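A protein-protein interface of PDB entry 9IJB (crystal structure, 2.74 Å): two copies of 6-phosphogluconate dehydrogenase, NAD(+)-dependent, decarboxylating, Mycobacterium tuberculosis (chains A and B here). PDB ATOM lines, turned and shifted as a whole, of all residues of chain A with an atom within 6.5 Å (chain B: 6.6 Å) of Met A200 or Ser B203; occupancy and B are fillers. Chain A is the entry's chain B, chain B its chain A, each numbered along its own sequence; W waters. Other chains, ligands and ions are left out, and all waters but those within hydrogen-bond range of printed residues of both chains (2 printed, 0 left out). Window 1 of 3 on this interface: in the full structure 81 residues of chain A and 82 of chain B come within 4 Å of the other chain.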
ATOM      1  N   GLY A 195     -36.501  -1.261  29.268  1.00  0.00           N
ATOM      2  CA  GLY A 195     -35.793  -1.726  30.452  1.00  0.00           C
ATOM      3  C   GLY A 195     -34.397  -2.212  30.112  1.00  0.00           C
ATOM      4  O   GLY A 195     -33.405  -1.756  30.684  1.00  0.00           O
ATOM      5  N   ILE A 196     -34.301  -3.119  29.138  1.00  0.00           N
ATOM      6  CA  ILE A 196     -33.002  -3.590  28.683  1.00  0.00           C
ATOM      7  C   ILE A 196     -32.150  -2.416  28.201  1.00  0.00           C
ATOM      8  O   ILE A 196     -30.924  -2.386  28.396  1.00  0.00           O
ATOM      9  CB  ILE A 196     -33.212  -4.664  27.595  1.00  0.00           C
ATOM     10  CG1 ILE A 196     -33.908  -5.898  28.181  1.00  0.00           C
ATOM     11  CG2 ILE A 196     -31.928  -5.076  26.927  1.00  0.00           C
ATOM     12  CD1 ILE A 196     -34.324  -6.912  27.100  1.00  0.00           C
ATOM     13  N   GLU A 197     -32.785  -1.421  27.581  1.00  0.00           N
ATOM     14  CA  GLU A 197     -32.061  -0.280  27.035  1.00  0.00           C
ATOM     15  C   GLU A 197     -31.442   0.551  28.151  1.00  0.00           C
ATOM     16  O   GLU A 197     -30.326   1.060  28.005  1.00  0.00           O
ATOM     17  CB  GLU A 197     -32.996   0.555  26.159  1.00  0.00           C
ATOM     18  CG  GLU A 197     -32.460   1.902  25.671  1.00  0.00           C
ATOM     19  CD  GLU A 197     -33.564   2.969  25.608  1.00  0.00           C
ATOM     20  OE1 GLU A 197     -33.904   3.532  26.672  1.00  0.00           O
ATOM     21  OE2 GLU A 197     -34.117   3.224  24.502  1.00  0.00           O
ATOM     22  N   TYR A 198     -32.174   0.719  29.256  1.00  0.00           N
ATOM     23  CA  TYR A 198     -31.608   1.457  30.381  1.00  0.00           C
ATOM     24  C   TYR A 198     -30.342   0.774  30.880  1.00  0.00           C
ATOM     25  O   TYR A 198     -29.371   1.447  31.253  1.00  0.00           O
ATOM     26  CB  TYR A 198     -32.601   1.564  31.539  1.00  0.00           C
ATOM     27  CG  TYR A 198     -33.756   2.536  31.390  1.00  0.00           C
ATOM     28  CD1 TYR A 198     -34.095   3.084  30.167  1.00  0.00           C
ATOM     29  CD2 TYR A 198     -34.509   2.908  32.506  1.00  0.00           C
ATOM     30  CE1 TYR A 198     -35.158   3.957  30.059  1.00  0.00           C
ATOM     31  CE2 TYR A 198     -35.564   3.780  32.401  1.00  0.00           C
ATOM     32  CZ  TYR A 198     -35.884   4.293  31.179  1.00  0.00           C
ATOM     33  OH  TYR A 198     -36.943   5.153  31.083  1.00  0.00           O
ATOM     34  N   GLY A 199     -30.344  -0.563  30.895  1.00  0.00           N
ATOM     35  CA  GLY A 199     -29.242  -1.293  31.500  1.00  0.00           C
ATOM     36  C   GLY A 199     -28.028  -1.365  30.593  1.00  0.00           C
ATOM     37  O   GLY A 199     -26.878  -1.421  31.061  1.00  0.00           O
ATOM     38  N   MET A 200     -28.252  -1.377  29.282  1.00  0.00           N
ATOM     39  CA  MET A 200     -27.120  -1.278  28.374  1.00  0.00           C
ATOM     40  C   MET A 200     -26.479   0.106  28.458  1.00  0.00           C
ATOM     41  O   MET A 200     -25.267   0.231  28.647  1.00  0.00           O
ATOM     42  CB  MET A 200     -27.569  -1.624  26.958  1.00  0.00           C
ATOM     43  CG  MET A 200     -28.024  -3.087  26.845  1.00  0.00           C
ATOM     44  SD  MET A 200     -28.523  -3.547  25.182  1.00  0.00           S
ATOM     45  CE  MET A 200     -27.084  -2.976  24.262  1.00  0.00           C
ATOM     46  N   MET A 201     -27.290   1.160  28.355  1.00  0.00           N
ATOM     47  CA  MET A 201     -26.797   2.524  28.519  1.00  0.00           C
ATOM     48  C   MET A 201     -25.966   2.664  29.787  1.00  0.00           C
ATOM     49  O   MET A 201     -24.800   3.071  29.742  1.00  0.00           O
ATOM     50  CB  MET A 201     -27.975   3.502  28.558  1.00  0.00           C
ATOM     51  CG  MET A 201     -28.787   3.631  27.280  1.00  0.00           C
ATOM     52  SD  MET A 201     -30.339   4.478  27.596  1.00  0.00           S
ATOM     53  CE  MET A 201     -29.810   6.154  27.837  1.00  0.00           C
ATOM     54  N   ALA A 202     -26.574   2.356  30.931  1.00  0.00           N
ATOM     55  CA  ALA A 202     -25.876   2.447  32.206  1.00  0.00           C
ATOM     56  C   ALA A 202     -24.620   1.591  32.238  1.00  0.00           C
ATOM     57  O   ALA A 202     -23.624   1.973  32.865  1.00  0.00           O
ATOM     58  CB  ALA A 202     -26.807   2.024  33.344  1.00  0.00           C
ATOM     59  N   SER A 203     -24.641   0.410  31.606  1.00  0.00           N
ATOM     60  CA  SER A 203     -23.439  -0.423  31.621  1.00  0.00           C
ATOM     61  C   SER A 203     -22.270   0.313  30.993  1.00  0.00           C
ATOM     62  O   SER A 203     -21.153   0.297  31.521  1.00  0.00           O
ATOM     63  CB  SER A 203     -23.691  -1.750  30.900  1.00  0.00           C
ATOM     64  OG  SER A 203     -24.472  -2.610  31.714  1.00  0.00           O
ATOM     65  N   LEU A 204     -22.536   1.029  29.911  1.00  0.00           N
ATOM     66  CA  LEU A 204     -21.408   1.677  29.273  1.00  0.00           C
ATOM     67  C   LEU A 204     -21.166   3.053  29.899  1.00  0.00           C
ATOM     68  O   LEU A 204     -20.025   3.471  30.109  1.00  0.00           O
ATOM     69  CB  LEU A 204     -21.668   1.721  27.748  1.00  0.00           C
ATOM     70  CG  LEU A 204     -20.802   2.744  27.061  1.00  0.00           C
ATOM     71  CD1 LEU A 204     -19.419   2.238  26.740  1.00  0.00           C
ATOM     72  CD2 LEU A 204     -21.559   2.952  25.810  1.00  0.00           C
ATOM     73  N   ALA A 205     -22.199   3.713  30.398  1.00  0.00           N
ATOM     74  CA  ALA A 205     -22.018   4.933  31.164  1.00  0.00           C
ATOM     75  C   ALA A 205     -21.117   4.708  32.368  1.00  0.00           C
ATOM     76  O   ALA A 205     -20.163   5.462  32.583  1.00  0.00           O
ATOM     77  CB  ALA A 205     -23.385   5.470  31.597  1.00  0.00           C
ATOM     78  N   GLY A 256     -19.762  -4.238  21.097  1.00  0.00           N
ATOM     79  CA  GLY A 256     -20.315  -3.428  20.019  1.00  0.00           C
ATOM     80  C   GLY A 256     -21.825  -3.321  20.115  1.00  0.00           C
ATOM     81  O   GLY A 256     -22.508  -4.233  20.592  1.00  0.00           O
ATOM     82  N   SER A 257     -22.354  -2.182  19.686  1.00  0.00           N
ATOM     83  CA  SER A 257     -23.773  -1.883  19.842  1.00  0.00           C
ATOM     84  C   SER A 257     -24.054  -0.517  19.242  1.00  0.00           C
ATOM     85  O   SER A 257     -23.171   0.348  19.172  1.00  0.00           O
ATOM     86  CB  SER A 257     -24.215  -1.864  21.306  1.00  0.00           C
ATOM     87  OG  SER A 257     -23.628  -0.765  22.010  1.00  0.00           O
ATOM     88  N   TRP A 258     -25.312  -0.328  18.836  1.00  0.00           N
ATOM     89  CA  TRP A 258     -25.753   0.966  18.334  1.00  0.00           C
ATOM     90  C   TRP A 258     -25.575   2.060  19.374  1.00  0.00           C
ATOM     91  O   TRP A 258     -25.252   3.199  19.016  1.00  0.00           O
ATOM     92  CB  TRP A 258     -27.205   0.883  17.923  1.00  0.00           C
ATOM     93  CG  TRP A 258     -27.637   2.007  17.114  1.00  0.00           C
ATOM     94  CD1 TRP A 258     -27.017   2.497  16.008  1.00  0.00           C
ATOM     95  CD2 TRP A 258     -28.804   2.801  17.315  1.00  0.00           C
ATOM     96  NE1 TRP A 258     -27.726   3.554  15.502  1.00  0.00           N
ATOM     97  CE2 TRP A 258     -28.831   3.761  16.286  1.00  0.00           C
ATOM     98  CE3 TRP A 258     -29.830   2.795  18.267  1.00  0.00           C
ATOM     99  CZ2 TRP A 258     -29.857   4.706  16.171  1.00  0.00           C
ATOM    100  CZ3 TRP A 258     -30.845   3.743  18.159  1.00  0.00           C
ATOM    101  CH2 TRP A 258     -30.847   4.684  17.114  1.00  0.00           C
ATOM    102  N   LEU A 259     -25.798   1.740  20.658  1.00  0.00           N
ATOM    103  CA  LEU A 259     -25.586   2.720  21.723  1.00  0.00           C
ATOM    104  C   LEU A 259     -24.129   3.124  21.807  1.00  0.00           C
ATOM    105  O   LEU A 259     -23.822   4.314  21.934  1.00  0.00           O
ATOM    106  CB  LEU A 259     -26.034   2.160  23.060  1.00  0.00           C
ATOM    107  CG  LEU A 259     -27.537   2.163  23.286  1.00  0.00           C
ATOM    108  CD1 LEU A 259     -27.828   1.388  24.548  1.00  0.00           C
ATOM    109  CD2 LEU A 259     -28.081   3.594  23.357  1.00  0.00           C
ATOM    110  N   VAL A 302     -29.830  -5.495  37.863  1.00  0.00           N
ATOM    111  CA  VAL A 302     -29.120  -4.752  36.863  1.00  0.00           C
ATOM    112  C   VAL A 302     -30.024  -3.794  36.161  1.00  0.00           C
ATOM    113  O   VAL A 302     -29.703  -2.648  36.025  1.00  0.00           O
ATOM    114  CB  VAL A 302     -28.488  -5.707  35.869  1.00  0.00           C
ATOM    115  CG1 VAL A 302     -27.523  -4.998  34.970  1.00  0.00           C
ATOM    116  CG2 VAL A 302     -27.774  -6.786  36.615  1.00  0.00           C
ATOM    117  N   LEU A 303     -31.186  -4.227  35.742  1.00  0.00           N
ATOM    118  CA  LEU A 303     -32.071  -3.224  35.146  1.00  0.00           C
ATOM    119  C   LEU A 303     -32.553  -2.203  36.180  1.00  0.00           C
ATOM    120  O   LEU A 303     -32.603  -1.007  35.891  1.00  0.00           O
ATOM    121  CB  LEU A 303     -33.268  -3.879  34.464  1.00  0.00           C
ATOM    122  CG  LEU A 303     -33.021  -4.774  33.239  1.00  0.00           C
ATOM    123  CD1 LEU A 303     -34.316  -4.967  32.485  1.00  0.00           C
ATOM    124  CD2 LEU A 303     -31.964  -4.198  32.320  1.00  0.00           C
ATOM    125  N   ALA A 306     -30.255   0.456  37.314  1.00  0.00           N
ATOM    126  CA  ALA A 306     -30.061   1.483  36.285  1.00  0.00           C
ATOM    127  C   ALA A 306     -31.133   2.580  36.363  1.00  0.00           C
ATOM    128  O   ALA A 306     -30.828   3.781  36.247  1.00  0.00           O
ATOM    129  CB  ALA A 306     -30.055   0.840  34.901  1.00  0.00           C
ATOM    130  N   ILE B 196     -18.175  -4.034  31.243  1.00  0.00           N
ATOM    131  CA  ILE B 196     -19.329  -3.594  30.463  1.00  0.00           C
ATOM    132  C   ILE B 196     -19.998  -4.784  29.777  1.00  0.00           C
ATOM    133  O   ILE B 196     -21.220  -4.811  29.602  1.00  0.00           O
ATOM    134  CB  ILE B 196     -18.894  -2.528  29.445  1.00  0.00           C
ATOM    135  CG1 ILE B 196     -18.248  -1.353  30.185  1.00  0.00           C
ATOM    136  CG2 ILE B 196     -20.069  -2.126  28.526  1.00  0.00           C
ATOM    137  CD1 ILE B 196     -17.604  -0.290  29.259  1.00  0.00           C
ATOM    138  N   TYR B 198     -20.345  -7.798  31.039  1.00  0.00           N
ATOM    139  CA  TYR B 198     -21.230  -8.380  32.044  1.00  0.00           C
ATOM    140  C   TYR B 198     -22.516  -7.572  32.167  1.00  0.00           C
ATOM    141  O   TYR B 198     -23.617  -8.124  32.145  1.00  0.00           O
ATOM    142  CB  TYR B 198     -20.517  -8.469  33.398  1.00  0.00           C
ATOM    143  CG  TYR B 198     -19.428  -9.526  33.472  1.00  0.00           C
ATOM    144  CD1 TYR B 198     -19.055 -10.237  32.355  1.00  0.00           C
ATOM    145  CD2 TYR B 198     -18.782  -9.810  34.674  1.00  0.00           C
ATOM    146  CE1 TYR B 198     -18.079 -11.186  32.412  1.00  0.00           C
ATOM    147  CE2 TYR B 198     -17.798 -10.762  34.750  1.00  0.00           C
ATOM    148  CZ  TYR B 198     -17.453 -11.458  33.611  1.00  0.00           C
ATOM    149  OH  TYR B 198     -16.463 -12.419  33.651  1.00  0.00           O
ATOM    150  N   GLY B 199     -22.391  -6.256  32.254  1.00  0.00           N
ATOM    151  CA  GLY B 199     -23.567  -5.431  32.454  1.00  0.00           C
ATOM    152  C   GLY B 199     -24.533  -5.550  31.301  1.00  0.00           C
ATOM    153  O   GLY B 199     -25.750  -5.572  31.496  1.00  0.00           O
ATOM    154  N   MET B 200     -24.005  -5.665  30.080  1.00  0.00           N
ATOM    155  CA  MET B 200     -24.893  -5.802  28.934  1.00  0.00           C
ATOM    156  C   MET B 200     -25.550  -7.178  28.872  1.00  0.00           C
ATOM    157  O   MET B 200     -26.746  -7.286  28.569  1.00  0.00           O
ATOM    158  CB  MET B 200     -24.157  -5.512  27.631  1.00  0.00           C
ATOM    159  CG  MET B 200     -23.615  -4.105  27.479  1.00  0.00           C
ATOM    160  SD  MET B 200     -22.529  -3.981  26.053  1.00  0.00           S
ATOM    161  CE  MET B 200     -23.747  -3.937  24.814  1.00  0.00           C
ATOM    162  N   MET B 201     -24.782  -8.239  29.082  1.00  0.00           N
ATOM    163  CA  MET B 201     -25.437  -9.542  29.063  1.00  0.00           C
ATOM    164  C   MET B 201     -26.487  -9.674  30.176  1.00  0.00           C
ATOM    165  O   MET B 201     -27.596 -10.171  29.941  1.00  0.00           O
ATOM    166  CB  MET B 201     -24.391 -10.652  29.147  1.00  0.00           C
ATOM    167  CG  MET B 201     -23.067 -10.284  28.569  1.00  0.00           C
ATOM    168  SD  MET B 201     -21.796 -11.273  29.318  1.00  0.00           S
ATOM    169  CE  MET B 201     -22.107 -12.950  28.738  1.00  0.00           C
ATOM    170  N   ALA B 202     -26.247  -9.125  31.373  1.00  0.00           N
ATOM    171  CA  ALA B 202     -27.246  -9.224  32.439  1.00  0.00           C
ATOM    172  C   ALA B 202     -28.511  -8.459  32.077  1.00  0.00           C
ATOM    173  O   ALA B 202     -29.627  -8.898  32.372  1.00  0.00           O
ATOM    174  CB  ALA B 202     -26.670  -8.697  33.761  1.00  0.00           C
ATOM    175  N   SER B 203     -28.352  -7.313  31.438  1.00  0.00           N
ATOM    176  CA  SER B 203     -29.515  -6.540  31.018  1.00  0.00           C
ATOM    177  C   SER B 203     -30.354  -7.322  30.014  1.00  0.00           C
ATOM    178  O   SER B 203     -31.585  -7.359  30.126  1.00  0.00           O
ATOM    179  CB  SER B 203     -29.056  -5.206  30.440  1.00  0.00           C
ATOM    180  OG  SER B 203     -28.344  -4.458  31.421  1.00  0.00           O
ATOM    181  N   LEU B 204     -29.701  -7.986  29.048  1.00  0.00           N
ATOM    182  CA  LEU B 204     -30.417  -8.892  28.150  1.00  0.00           C
ATOM    183  C   LEU B 204     -31.061 -10.042  28.916  1.00  0.00           C
ATOM    184  O   LEU B 204     -32.230 -10.379  28.678  1.00  0.00           O
ATOM    185  CB  LEU B 204     -29.477  -9.455  27.089  1.00  0.00           C
ATOM    186  CG  LEU B 204     -29.340  -8.599  25.825  1.00  0.00           C
ATOM    187  CD1 LEU B 204     -28.473  -9.298  24.779  1.00  0.00           C
ATOM    188  CD2 LEU B 204     -30.687  -8.283  25.268  1.00  0.00           C
ATOM    189  N   ALA B 205     -30.318 -10.658  29.837  1.00  0.00           N
ATOM    190  CA  ALA B 205     -30.807 -11.866  30.478  1.00  0.00           C
ATOM    191  C   ALA B 205     -31.977 -11.551  31.390  1.00  0.00           C
ATOM    192  O   ALA B 205     -32.993 -12.255  31.375  1.00  0.00           O
ATOM    193  CB  ALA B 205     -29.680 -12.551  31.251  1.00  0.00           C
ATOM    194  N   GLU B 206     -31.853 -10.493  32.194  1.00  0.00           N
ATOM    195  CA  GLU B 206     -32.942 -10.117  33.085  1.00  0.00           C
ATOM    196  C   GLU B 206     -34.210  -9.814  32.301  1.00  0.00           C
ATOM    197  O   GLU B 206     -35.298 -10.263  32.681  1.00  0.00           O
ATOM    198  CB  GLU B 206     -32.559  -8.912  33.935  1.00  0.00           C
ATOM    199  CG  GLU B 206     -31.555  -9.179  35.041  1.00  0.00           C
ATOM    200  CD  GLU B 206     -31.249  -7.932  35.900  1.00  0.00           C
ATOM    201  OE1 GLU B 206     -30.498  -8.088  36.863  1.00  0.00           O
ATOM    202  OE2 GLU B 206     -31.740  -6.792  35.653  1.00  0.00           O
ATOM    203  N   GLY B 207     -34.094  -9.050  31.205  1.00  0.00           N
ATOM    204  CA  GLY B 207     -35.232  -8.739  30.356  1.00  0.00           C
ATOM    205  C   GLY B 207     -35.919  -9.982  29.815  1.00  0.00           C
ATOM    206  O   GLY B 207     -37.114 -10.187  30.041  1.00  0.00           O
ATOM    207  N   LEU B 208     -35.162 -10.831  29.112  1.00  0.00           N
ATOM    208  CA  LEU B 208     -35.604 -12.160  28.722  1.00  0.00           C
ATOM    209  C   LEU B 208     -36.363 -12.867  29.845  1.00  0.00           C
ATOM    210  O   LEU B 208     -37.375 -13.540  29.606  1.00  0.00           O
ATOM    211  CB  LEU B 208     -34.400 -12.980  28.294  1.00  0.00           C
ATOM    212  CG  LEU B 208     -33.730 -12.535  26.980  1.00  0.00           C
ATOM    213  CD1 LEU B 208     -32.679 -13.542  26.497  1.00  0.00           C
ATOM    214  CD2 LEU B 208     -34.717 -12.234  25.840  1.00  0.00           C
ATOM    215  N   VAL B 254     -33.210   0.194  19.603  1.00  0.00           N
ATOM    216  CA  VAL B 254     -32.110   0.893  20.265  1.00  0.00           C
ATOM    217  C   VAL B 254     -31.086  -0.060  20.885  1.00  0.00           C
ATOM    218  O   VAL B 254     -29.948   0.352  21.166  1.00  0.00           O
ATOM    219  CB  VAL B 254     -32.694   1.825  21.350  1.00  0.00           C
ATOM    220  CG1 VAL B 254     -31.647   2.808  21.872  1.00  0.00           C
ATOM    221  CG2 VAL B 254     -33.874   2.577  20.808  1.00  0.00           C
ATOM    222  N   ILE B 255     -31.450  -1.321  21.117  1.00  0.00           N
ATOM    223  CA  ILE B 255     -30.566  -2.262  21.793  1.00  0.00           C
ATOM    224  C   ILE B 255     -29.854  -3.178  20.795  1.00  0.00           C
ATOM    225  O   ILE B 255     -29.312  -4.209  21.184  1.00  0.00           O
ATOM    226  CB  ILE B 255     -31.309  -3.072  22.871  1.00  0.00           C
ATOM    227  CG1 ILE B 255     -32.336  -4.004  22.238  1.00  0.00           C
ATOM    228  CG2 ILE B 255     -32.009  -2.156  23.837  1.00  0.00           C
ATOM    229  CD1 ILE B 255     -33.282  -4.597  23.245  1.00  0.00           C
ATOM    230  N   GLY B 256     -29.829  -2.807  19.523  1.00  0.00           N
ATOM    231  CA  GLY B 256     -29.003  -3.506  18.567  1.00  0.00           C
ATOM    232  C   GLY B 256     -27.598  -3.662  19.110  1.00  0.00           C
ATOM    233  O   GLY B 256     -27.055  -2.708  19.675  1.00  0.00           O
ATOM    234  N   SER B 257     -27.019  -4.860  18.973  1.00  0.00           N
ATOM    235  CA  SER B 257     -25.716  -5.189  19.530  1.00  0.00           C
ATOM    236  C   SER B 257     -25.302  -6.583  19.074  1.00  0.00           C
ATOM    237  O   SER B 257     -26.138  -7.431  18.757  1.00  0.00           O
ATOM    238  CB  SER B 257     -25.740  -5.132  21.058  1.00  0.00           C
ATOM    239  OG  SER B 257     -26.240  -6.342  21.611  1.00  0.00           O
ATOM    240  N   LEU B 260     -26.882  -9.205  21.432  1.00  0.00           N
ATOM    241  CA  LEU B 260     -28.244  -9.579  21.046  1.00  0.00           C
ATOM    242  C   LEU B 260     -28.235 -10.536  19.853  1.00  0.00           C
ATOM    243  O   LEU B 260     -28.903 -11.573  19.869  1.00  0.00           O
ATOM    244  CB  LEU B 260     -29.087  -8.335  20.743  1.00  0.00           C
ATOM    245  CG  LEU B 260     -30.525  -8.610  20.263  1.00  0.00           C
ATOM    246  CD1 LEU B 260     -31.431  -8.892  21.445  1.00  0.00           C
ATOM    247  CD2 LEU B 260     -31.112  -7.443  19.492  1.00  0.00           C
ATOM    248  N   VAL B 302     -24.768  -0.914  38.371  1.00  0.00           N
ATOM    249  CA  VAL B 302     -25.206  -1.772  37.276  1.00  0.00           C
ATOM    250  C   VAL B 302     -24.162  -2.838  36.968  1.00  0.00           C
ATOM    251  O   VAL B 302     -24.492  -4.027  36.849  1.00  0.00           O
ATOM    252  CB  VAL B 302     -25.569  -0.957  36.030  1.00  0.00           C
ATOM    253  CG1 VAL B 302     -26.112  -1.894  34.960  1.00  0.00           C
ATOM    254  CG2 VAL B 302     -26.613   0.101  36.367  1.00  0.00           C
ATOM    255  N   ALA B 306     -24.471  -6.980  38.212  1.00  0.00           N
ATOM    256  CA  ALA B 306     -24.370  -8.023  37.193  1.00  0.00           C
ATOM    257  C   ALA B 306     -23.353  -9.072  37.588  1.00  0.00           C
ATOM    258  O   ALA B 306     -23.592 -10.282  37.454  1.00  0.00           O
ATOM    259  CB  ALA B 306     -23.985  -7.425  35.841  1.00  0.00           C
HETATM  260  O   HOH W   1     -27.709  -0.848  21.411  1.00  0.00           O
HETATM  261  O   HOH W   2     -27.303  -3.492  38.848  1.00  0.00           O
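OE1 of Glu B206 sits at hydrogen-bond distance from N of Val A302, at 2.9 Å.
The backbone NH (N) of Leu A303 sits at hydrogen-bond distance from the side-chain carboxylate (OE2) of Glu B206 (2.6 Å).
O of Gly B199 sits close to OG of Ser A203 (3.2 Å).
The backbone carbonyl oxygen of Gly B256 sits at hydrogen-bond distance from the backbone NH of Trp A258, at 3.1 Å.
The side-chain hydroxyl (OG) of Ser B203 lies close to the backbone carbonyl oxygen (O) of Gly A199, 3.4 Å away.
The backbone NH (N) of Met B200 is in hydrogen-bond range of the side-chain hydroxyl (OG) of Ser A203, 3.5 Å away.
The backbone NH (N) of Leu B260 sits at hydrogen-bond distance from the side-chain hydroxyl (OG) of Ser B257, at 2.9 Å.
The backbone carbonyl oxygen of Gly B199 is in hydrogen-bond range of the side-chain hydroxyl of Ser B203 (2.8 Å).
The side-chain hydroxyl of Ser A203 is in hydrogen-bond range of the backbone carbonyl oxygen of Gly A199, at 2.8 Å.
Among the printed residues, merely in contact across the chains: Ile A196 with Ser B203 (3.4 Å), Ile A196 with Leu B204 (3.8 Å), Ile A196 with Gly B207 (3.8 Å), Ile A196 with Ile B255 (3.95 Å), Glu A197 with Val B254 (3.6 Å), Glu A197 with Ile B255 (3.7 Å), Met A200 with Met B200 (3.5 Å), Met A200 with Ser B203 (3.8 Å), Met A200 with Ile B255 (3.7 Å), Ala A202 with Val B302 (3.6 Å), Ser A203 with Ile B196 (3.6 Å), Ser A203 with Val B302 (3.7 Å), Gly A256 with Ser B257 (3.4 Å), Ser A257 with Gly B256 (3.4 Å), Ser A257 with Ser B257 (3.6 Å), Trp A258 with Val B254 (3.6 Å), Leu A259 with Val B254 (3.7 Å), Val A302 with Gly B199 (3.9 Å), Val A302 with Ala B202 (3.6 Å), Val A302 with Ser B203 (3.7 Å), Val A302 with Val B302 (3.4 Å), Val A302 with Ala B306 (3.7 Å), Leu A303 with Ser B203 (3.6 Å) and Ala A306 with Val B302 (3.7 Å).
Of the printed residues of chain B, Met A200 touches Met B200, Ser B203 and Ile B255.
Ser B203 touches just these residues of chain A: Ile A196 (3.4 Å), Gly A199 (3.2 Å), Met A200 (3.8 Å), Val A302 (3.7 Å) and Leu A303 (3.6 Å).
Printed residues of chain B within 4 Å of Ser A203: Ile B196 (3.6 Å), Gly B199 (3.0 Å), Met B200 (3.5 Å) and Val B302 (3.7 Å).
Printed residues of chain B within 4 Å of Trp A258: Val B254 (3.6 Å) and Gly B256 (3.1 Å).
Of the printed residues of chain B, Ile A196 touches Ser B203 (3.4 Å), Leu B204 (3.8 Å), Gly B207 (3.8 Å) and Ile B255 (3.95 Å).
Of the 19 printed residues of chain B, 14 touch a printed residue of chain A.
Hydrophobic or aromatic side chains of chain B within 4 Å of the printed part of chain A: Ile B196, Met B200, Ala B202, Leu B204, Val B254, Ile B255, Val B302 and Ala B306.
Of the 18 printed residues of chain A, 13 touch a printed residue of chain B.
Hydrophobic or aromatic side chains of chain A that line the printed part of chain B: Ile A196, Met A200, Ala A202, Trp A258, Leu A259, Val A302, Leu A303 and Ala A306.
Among the printed residues, 30 pairs touch across the chains.
Ile A196 touches Ser B203, and with the chains exchanged Ser A203 touches Ile B196.
Gly A199 touches Ser B203, and with the chains exchanged Ser A203 touches Gly B199.
Ala A202 touches Val B302, and with the chains exchanged Val A302 touches Ala B202.
Val A302 touches Gly B199, but with the chains exchanged Gly A199 does not touch Val B302 (4.002 Å).
Of the 30 pairs that touch across the chains among the printed residues, 17 have their exchanged pair printed and touching as well.
Water W1 lies within hydrogen-bond range of O of Val B254 (2.6 Å), O of Gly B256 (2.6 Å) and N of Leu A259 (3.3 Å).
Water W2 bridges the backbone NH (N) of Val A302 (3.4 Å) and the backbone carbonyl oxygen (O) of Val B302 (3.5 Å).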
